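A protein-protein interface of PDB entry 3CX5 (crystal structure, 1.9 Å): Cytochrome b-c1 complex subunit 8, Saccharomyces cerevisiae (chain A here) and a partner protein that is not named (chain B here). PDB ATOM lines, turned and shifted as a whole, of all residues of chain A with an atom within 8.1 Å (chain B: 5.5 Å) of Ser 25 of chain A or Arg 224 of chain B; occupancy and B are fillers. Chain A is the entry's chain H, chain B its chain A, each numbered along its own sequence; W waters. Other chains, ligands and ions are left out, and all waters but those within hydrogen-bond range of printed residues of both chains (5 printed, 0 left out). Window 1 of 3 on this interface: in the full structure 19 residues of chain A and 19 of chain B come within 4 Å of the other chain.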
ATOM      1  N   TRP A  12      32.902 -25.883 -34.188  1.00  0.00           N
ATOM      2  CA  TRP A  12      32.361 -26.502 -32.976  1.00  0.00           C
ATOM      3  C   TRP A  12      33.193 -27.712 -32.525  1.00  0.00           C
ATOM      4  O   TRP A  12      33.442 -28.640 -33.304  1.00  0.00           O
ATOM      5  CB  TRP A  12      30.900 -26.900 -33.197  1.00  0.00           C
ATOM      6  CG  TRP A  12      29.996 -25.757 -33.608  1.00  0.00           C
ATOM      7  CD1 TRP A  12      29.474 -25.534 -34.848  1.00  0.00           C
ATOM      8  CD2 TRP A  12      29.520 -24.684 -32.776  1.00  0.00           C
ATOM      9  NE1 TRP A  12      28.710 -24.393 -34.845  1.00  0.00           N
ATOM     10  CE2 TRP A  12      28.720 -23.851 -33.587  1.00  0.00           C
ATOM     11  CE3 TRP A  12      29.699 -24.346 -31.428  1.00  0.00           C
ATOM     12  CZ2 TRP A  12      28.100 -22.698 -33.100  1.00  0.00           C
ATOM     13  CZ3 TRP A  12      29.079 -23.195 -30.940  1.00  0.00           C
ATOM     14  CH2 TRP A  12      28.290 -22.387 -31.777  1.00  0.00           C
ATOM     15  N   GLY A  22      35.953 -24.490 -14.690  1.00  0.00           N
ATOM     16  CA  GLY A  22      35.501 -23.727 -13.537  1.00  0.00           C
ATOM     17  C   GLY A  22      34.306 -22.820 -13.786  1.00  0.00           C
ATOM     18  O   GLY A  22      33.733 -22.262 -12.844  1.00  0.00           O
ATOM     19  N   ILE A  23      33.936 -22.646 -15.051  1.00  0.00           N
ATOM     20  CA  ILE A  23      32.794 -21.805 -15.389  1.00  0.00           C
ATOM     21  C   ILE A  23      31.569 -22.682 -15.576  1.00  0.00           C
ATOM     22  O   ILE A  23      31.624 -23.696 -16.274  1.00  0.00           O
ATOM     23  CB  ILE A  23      33.019 -21.026 -16.700  1.00  0.00           C
ATOM     24  CG1 ILE A  23      34.378 -20.322 -16.682  1.00  0.00           C
ATOM     25  CG2 ILE A  23      31.902 -20.010 -16.909  1.00  0.00           C
ATOM     26  CD1 ILE A  23      34.722 -19.640 -17.996  1.00  0.00           C
ATOM     27  N   THR A  24      30.478 -22.307 -14.923  1.00  0.00           N
ATOM     28  CA  THR A  24      29.219 -23.026 -15.042  1.00  0.00           C
ATOM     29  C   THR A  24      28.176 -22.026 -15.552  1.00  0.00           C
ATOM     30  O   THR A  24      28.104 -20.898 -15.062  1.00  0.00           O
ATOM     31  CB  THR A  24      28.763 -23.583 -13.682  1.00  0.00           C
ATOM     32  OG1 THR A  24      29.765 -24.468 -13.169  1.00  0.00           O
ATOM     33  CG2 THR A  24      27.440 -24.340 -13.816  1.00  0.00           C
ATOM     34  N   SER A  25      27.420 -22.405 -16.577  1.00  0.00           N
ATOM     35  CA  SER A  25      26.389 -21.521 -17.115  1.00  0.00           C
ATOM     36  C   SER A  25      25.016 -22.149 -16.904  1.00  0.00           C
ATOM     37  O   SER A  25      24.888 -23.367 -16.856  1.00  0.00           O
ATOM     38  CB  SER A  25      26.621 -21.227 -18.604  1.00  0.00           C
ATOM     39  OG  SER A  25      26.385 -22.369 -19.410  1.00  0.00           O
ATOM     40  N   TYR A  26      24.010 -21.300 -16.736  1.00  0.00           N
ATOM     41  CA  TYR A  26      22.635 -21.734 -16.519  1.00  0.00           C
ATOM     42  C   TYR A  26      21.734 -20.915 -17.424  1.00  0.00           C
ATOM     43  O   TYR A  26      21.978 -19.729 -17.640  1.00  0.00           O
ATOM     44  CB  TYR A  26      22.208 -21.466 -15.071  1.00  0.00           C
ATOM     45  CG  TYR A  26      23.097 -22.062 -14.007  1.00  0.00           C
ATOM     46  CD1 TYR A  26      24.227 -21.378 -13.555  1.00  0.00           C
ATOM     47  CD2 TYR A  26      22.782 -23.288 -13.412  1.00  0.00           C
ATOM     48  CE1 TYR A  26      25.016 -21.898 -12.531  1.00  0.00           C
ATOM     49  CE2 TYR A  26      23.565 -23.816 -12.388  1.00  0.00           C
ATOM     50  CZ  TYR A  26      24.679 -23.114 -11.954  1.00  0.00           C
ATOM     51  OH  TYR A  26      25.467 -23.622 -10.951  1.00  0.00           O
ATOM     52  N   ALA A  27      20.673 -21.540 -17.920  1.00  0.00           N
ATOM     53  CA  ALA A  27      19.721 -20.862 -18.781  1.00  0.00           C
ATOM     54  C   ALA A  27      18.360 -21.488 -18.573  1.00  0.00           C
ATOM     55  O   ALA A  27      18.253 -22.616 -18.096  1.00  0.00           O
ATOM     56  CB  ALA A  27      20.135 -20.967 -20.274  1.00  0.00           C
ATOM     57  N   VAL A  28      17.330 -20.739 -18.942  1.00  0.00           N
ATOM     58  CA  VAL A  28      15.952 -21.182 -18.814  1.00  0.00           C
ATOM     59  C   VAL A  28      15.281 -21.065 -20.174  1.00  0.00           C
ATOM     60  O   VAL A  28      15.561 -20.144 -20.939  1.00  0.00           O
ATOM     61  CB  VAL A  28      15.188 -20.309 -17.776  1.00  0.00           C
ATOM     62  CG1 VAL A  28      13.701 -20.617 -17.807  1.00  0.00           C
ATOM     63  CG2 VAL A  28      15.733 -20.560 -16.385  1.00  0.00           C
ATOM     64  N   GLU B 222      18.778 -25.558 -18.446  1.00  0.00           N
ATOM     65  CA  GLU B 222      20.044 -26.250 -18.627  1.00  0.00           C
ATOM     66  C   GLU B 222      21.138 -25.723 -17.713  1.00  0.00           C
ATOM     67  O   GLU B 222      21.099 -24.581 -17.260  1.00  0.00           O
ATOM     68  CB  GLU B 222      20.522 -26.102 -20.074  1.00  0.00           C
ATOM     69  CG  GLU B 222      20.743 -24.639 -20.486  1.00  0.00           C
ATOM     70  CD  GLU B 222      21.344 -24.486 -21.872  1.00  0.00           C
ATOM     71  OE1 GLU B 222      22.045 -23.482 -22.108  1.00  0.00           O
ATOM     72  OE2 GLU B 222      21.120 -25.363 -22.729  1.00  0.00           O
ATOM     73  N   VAL B 223      22.094 -26.595 -17.426  1.00  0.00           N
ATOM     74  CA  VAL B 223      23.253 -26.258 -16.627  1.00  0.00           C
ATOM     75  C   VAL B 223      24.416 -26.887 -17.392  1.00  0.00           C
ATOM     76  O   VAL B 223      24.374 -28.067 -17.749  1.00  0.00           O
ATOM     77  CB  VAL B 223      23.157 -26.778 -15.156  1.00  0.00           C
ATOM     78  CG1 VAL B 223      22.808 -28.259 -15.103  1.00  0.00           C
ATOM     79  CG2 VAL B 223      24.470 -26.519 -14.430  1.00  0.00           C
ATOM     80  N   ARG B 224      25.406 -26.063 -17.716  1.00  0.00           N
ATOM     81  CA  ARG B 224      26.566 -26.502 -18.473  1.00  0.00           C
ATOM     82  C   ARG B 224      27.828 -26.351 -17.632  1.00  0.00           C
ATOM     83  O   ARG B 224      28.167 -25.252 -17.185  1.00  0.00           O
ATOM     84  CB  ARG B 224      26.643 -25.705 -19.788  1.00  0.00           C
ATOM     85  CG  ARG B 224      25.399 -25.923 -20.674  1.00  0.00           C
ATOM     86  CD  ARG B 224      25.228 -24.896 -21.791  1.00  0.00           C
ATOM     87  NE  ARG B 224      25.689 -25.407 -23.071  1.00  0.00           N
ATOM     88  CZ  ARG B 224      24.914 -25.682 -24.116  1.00  0.00           C
ATOM     89  NH1 ARG B 224      25.472 -26.149 -25.212  1.00  0.00           N
ATOM     90  NH2 ARG B 224      23.603 -25.477 -24.092  1.00  0.00           N
ATOM     91  N   LEU B 225      28.471 -27.486 -17.370  1.00  0.00           N
ATOM     92  CA  LEU B 225      29.685 -27.560 -16.565  1.00  0.00           C
ATOM     93  C   LEU B 225      30.864 -27.900 -17.468  1.00  0.00           C
ATOM     94  O   LEU B 225      31.512 -28.942 -17.302  1.00  0.00           O
ATOM     95  CB  LEU B 225      29.526 -28.655 -15.504  1.00  0.00           C
ATOM     96  CG  LEU B 225      28.311 -28.571 -14.572  1.00  0.00           C
ATOM     97  CD1 LEU B 225      27.850 -29.966 -14.187  1.00  0.00           C
ATOM     98  CD2 LEU B 225      28.649 -27.757 -13.336  1.00  0.00           C
ATOM     99  N   ARG B 226      31.155 -27.015 -18.415  1.00  0.00           N
ATOM    100  CA  ARG B 226      32.248 -27.262 -19.340  1.00  0.00           C
ATOM    101  C   ARG B 226      33.594 -27.448 -18.655  1.00  0.00           C
ATOM    102  O   ARG B 226      33.945 -26.709 -17.739  1.00  0.00           O
ATOM    103  CB  ARG B 226      32.383 -26.148 -20.382  1.00  0.00           C
ATOM    104  CG  ARG B 226      33.062 -26.669 -21.639  1.00  0.00           C
ATOM    105  CD  ARG B 226      34.023 -25.706 -22.279  1.00  0.00           C
ATOM    106  NE  ARG B 226      33.393 -24.822 -23.241  1.00  0.00           N
ATOM    107  CZ  ARG B 226      33.986 -24.354 -24.340  1.00  0.00           C
ATOM    108  NH1 ARG B 226      33.318 -23.535 -25.135  1.00  0.00           N
ATOM    109  NH2 ARG B 226      35.223 -24.719 -24.666  1.00  0.00           N
ATOM    110  N   ILE B 407      18.620 -29.948 -19.692  1.00  0.00           N
ATOM    111  CA  ILE B 407      19.905 -30.443 -20.166  1.00  0.00           C
ATOM    112  C   ILE B 407      20.995 -30.194 -19.145  1.00  0.00           C
ATOM    113  O   ILE B 407      21.006 -29.159 -18.474  1.00  0.00           O
ATOM    114  CB  ILE B 407      20.352 -29.721 -21.485  1.00  0.00           C
ATOM    115  CG1 ILE B 407      19.191 -29.605 -22.473  1.00  0.00           C
ATOM    116  CG2 ILE B 407      21.489 -30.484 -22.141  1.00  0.00           C
ATOM    117  CD1 ILE B 407      19.527 -28.788 -23.719  1.00  0.00           C
ATOM    118  N   GLY B 409      25.425 -31.097 -18.720  1.00  0.00           N
ATOM    119  CA  GLY B 409      26.600 -31.637 -19.381  1.00  0.00           C
ATOM    120  C   GLY B 409      27.914 -31.172 -18.784  1.00  0.00           C
ATOM    121  O   GLY B 409      27.984 -30.103 -18.169  1.00  0.00           O
ATOM    122  N   ILE B 413      32.079 -30.069 -23.974  1.00  0.00           N
ATOM    123  CA  ILE B 413      30.760 -29.800 -24.523  1.00  0.00           C
ATOM    124  C   ILE B 413      30.637 -28.535 -25.378  1.00  0.00           C
ATOM    125  O   ILE B 413      29.535 -28.034 -25.595  1.00  0.00           O
ATOM    126  CB  ILE B 413      29.688 -29.774 -23.403  1.00  0.00           C
ATOM    127  CG1 ILE B 413      30.075 -28.763 -22.317  1.00  0.00           C
ATOM    128  CG2 ILE B 413      29.507 -31.167 -22.823  1.00  0.00           C
ATOM    129  CD1 ILE B 413      29.010 -28.551 -21.250  1.00  0.00           C
ATOM    130  N   LEU B 416      28.154 -28.911 -28.037  1.00  0.00           N
ATOM    131  CA  LEU B 416      26.729 -29.033 -27.712  1.00  0.00           C
ATOM    132  C   LEU B 416      26.156 -27.645 -28.004  1.00  0.00           C
ATOM    133  O   LEU B 416      26.547 -26.664 -27.373  1.00  0.00           O
ATOM    134  CB  LEU B 416      26.531 -29.390 -26.235  1.00  0.00           C
ATOM    135  CG  LEU B 416      25.086 -29.543 -25.726  1.00  0.00           C
ATOM    136  CD1 LEU B 416      24.417 -30.723 -26.403  1.00  0.00           C
ATOM    137  CD2 LEU B 416      25.082 -29.724 -24.206  1.00  0.00           C
ATOM    138  N   LEU B 417      25.279 -27.554 -29.000  1.00  0.00           N
ATOM    139  CA  LEU B 417      24.685 -26.274 -29.386  1.00  0.00           C
ATOM    140  C   LEU B 417      23.807 -25.649 -28.298  1.00  0.00           C
ATOM    141  O   LEU B 417      23.576 -26.246 -27.250  1.00  0.00           O
ATOM    142  CB  LEU B 417      23.895 -26.431 -30.691  1.00  0.00           C
ATOM    143  CG  LEU B 417      24.633 -26.258 -32.030  1.00  0.00           C
ATOM    144  CD1 LEU B 417      26.091 -26.660 -31.935  1.00  0.00           C
ATOM    145  CD2 LEU B 417      23.924 -27.040 -33.124  1.00  0.00           C
ATOM    146  N   ASP B 418      23.367 -24.425 -28.559  1.00  0.00           N
ATOM    147  CA  ASP B 418      22.519 -23.642 -27.671  1.00  0.00           C
ATOM    148  C   ASP B 418      21.204 -24.367 -27.369  1.00  0.00           C
ATOM    149  O   ASP B 418      20.758 -25.223 -28.147  1.00  0.00           O
ATOM    150  CB  ASP B 418      22.188 -22.333 -28.368  1.00  0.00           C
ATOM    151  CG  ASP B 418      21.529 -22.566 -29.715  1.00  0.00           C
ATOM    152  OD1 ASP B 418      22.233 -22.995 -30.653  1.00  0.00           O
ATOM    153  OD2 ASP B 418      20.299 -22.381 -29.825  1.00  0.00           O
ATOM    154  N   TYR B 419      20.546 -23.946 -26.291  1.00  0.00           N
ATOM    155  CA  TYR B 419      19.281 -24.551 -25.876  1.00  0.00           C
ATOM    156  C   TYR B 419      18.232 -24.620 -26.988  1.00  0.00           C
ATOM    157  O   TYR B 419      17.676 -25.683 -27.250  1.00  0.00           O
ATOM    158  CB  TYR B 419      18.698 -23.801 -24.668  1.00  0.00           C
ATOM    159  CG  TYR B 419      17.450 -24.452 -24.092  1.00  0.00           C
ATOM    160  CD1 TYR B 419      17.551 -25.459 -23.134  1.00  0.00           C
ATOM    161  CD2 TYR B 419      16.175 -24.087 -24.535  1.00  0.00           C
ATOM    162  CE1 TYR B 419      16.410 -26.097 -22.627  1.00  0.00           C
ATOM    163  CE2 TYR B 419      15.025 -24.722 -24.032  1.00  0.00           C
ATOM    164  CZ  TYR B 419      15.156 -25.727 -23.078  1.00  0.00           C
ATOM    165  OH  TYR B 419      14.033 -26.373 -22.579  1.00  0.00           O
ATOM    166  N   ILE B 422      18.563 -27.255 -29.734  1.00  0.00           N
ATOM    167  CA  ILE B 422      18.249 -28.576 -29.226  1.00  0.00           C
ATOM    168  C   ILE B 422      16.738 -28.682 -29.029  1.00  0.00           C
ATOM    169  O   ILE B 422      16.121 -29.654 -29.465  1.00  0.00           O
ATOM    170  CB  ILE B 422      18.999 -28.850 -27.920  1.00  0.00           C
ATOM    171  CG1 ILE B 422      20.506 -28.717 -28.164  1.00  0.00           C
ATOM    172  CG2 ILE B 422      18.653 -30.232 -27.405  1.00  0.00           C
ATOM    173  CD1 ILE B 422      21.365 -28.986 -26.946  1.00  0.00           C
HETATM  174  O   HOH W   1      30.258 -24.236 -18.633  1.00  0.00           O
HETATM  175  O   HOH W   2      34.356 -23.952 -17.625  1.00  0.00           O
HETATM  176  O   HOH W   3      19.002 -23.322 -15.194  1.00  0.00           O
HETATM  177  O   HOH W   4      23.967 -21.682 -20.718  1.00  0.00           O
HETATM  178  O   HOH W   5      34.353 -26.702 -15.103  1.00  0.00           O
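NH2 of Arg 224 of chain B lies within salt-bridge range of OE2 of Glu 222 of chain B, 2.8 Å away.
The backbone NH of Val 223 of chain B lies within hydrogen-bond range of the backbone carbonyl oxygen of Ile 407 of chain B (3.0 Å).
O of Val 223 of chain B is in hydrogen-bond range of N of Gly 409 of chain B (3.4 Å).
The guanidinium group (NH1) of Arg 224 of chain B is in hydrogen-bond range of the backbone carbonyl oxygen (O) of Leu 416 of chain B (2.5 Å).
NH1 of Arg 224 of chain B is in hydrogen-bond range of O of Leu 417 of chain B.
O of Gly 409 of chain B sits at hydrogen-bond distance from N of Leu 225 of chain B, 2.8 Å away.
Arg 224 of chain B touches Ile 23 of chain A.
Arg 226 of chain B touches Ile 23 of chain A.
Thr 24 of chain A touches Val 223 of chain B (CG2 to CG2, 3.7 Å).
Thr 24 of chain A touches Arg 224 of chain B (CA to O, 3.3 Å).
Thr 24 of chain A touches Leu 225 of chain B (OG1 to CD2, 3.5 Å).
O of Ser 25 of chain A touches O of Glu 222 of chain B (3.999 Å).
Ser 25 of chain A touches Val 223 of chain B (O to CA, 3.3 Å).
CA of Tyr 26 of chain A touches O of Glu 222 of chain B (3.3 Å).
Tyr 26 of chain A touches Val 223 of chain B (CE2 to CG2, 3.5 Å).
O of Ala 27 of chain A sits at hydrogen-bond distance from N of Glu 222 of chain B (3.0 Å).
N of Arg 224 of chain B is in hydrogen-bond range of O of Ser 25 of chain A, at 2.9 Å.
Water W5 bridges the backbone carbonyl oxygen of Arg 226 of chain B (2.7 Å) and the backbone NH of Gly 22 of chain A (2.8 Å).
Water W1 lies within hydrogen-bond range of the backbone carbonyl oxygen (O) of Arg 224 of chain B (2.7 Å), the backbone carbonyl oxygen (O) of Ile 23 of chain A (2.8 Å) and the backbone NH (N) of Arg 226 of chain B (2.9 Å).
Water W2 lies within hydrogen-bond range of the backbone carbonyl oxygen of Arg 226 of chain B (2.8 Å), the backbone NH of Ile 23 of chain A (2.9 Å) and the backbone NH of Gly 22 of chain A (3.4 Å).
Water W4 lies within hydrogen-bond range of OG of Ser 25 of chain A (2.8 Å) and OE1 of Glu 222 of chain B (3.0 Å).
Water W3 lies within hydrogen-bond range of the backbone carbonyl oxygen of Ala 27 of chain A (3.1 Å) and the backbone carbonyl oxygen of Glu 222 of chain B (3.2 Å).
Of the 13 printed residues of chain B, 5 touch a printed residue of chain A.
Hydrophobic or aromatic side chains of chain B that line the printed part of chain A: Val 223 and Leu 225.
Hydrophobic or aromatic side chains of chain A that line the printed part of chain B: Tyr 26 and Ala 27.
Among the printed residues, 11 pairs touch across the chains.
Of the printed residues of chain B, Thr 24 of chain A touches Val 223 (3.7 Å), Arg 224 (3.3 Å) and Leu 225 (3.5 Å).
Printed residues of chain B within 4 Å of Ser 25 of chain A: Glu 222 (3.999 Å), Val 223 (3.3 Å) and Arg 224 (2.9 Å).
Arg 224 of chain B touches just these residues of chain A: Ile 23, Thr 24 and Ser 25.
Printed residues of chain A within 4 Å of Arg 226 of chain B: Ile 23 (3.98 Å).
Gly 409 of chain B touches none of the printed residues of chain A.
Asp 418 of chain B touches none of the printed residues of chain A.
The nearest printed residue of chain B that does not touch Ser 25 of chain A is Leu 225 of chain B (5.2 Å).
The nearest printed residue of chain A that does not touch Val 223 of chain B is Ala 27 of chain A (5.3 Å).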
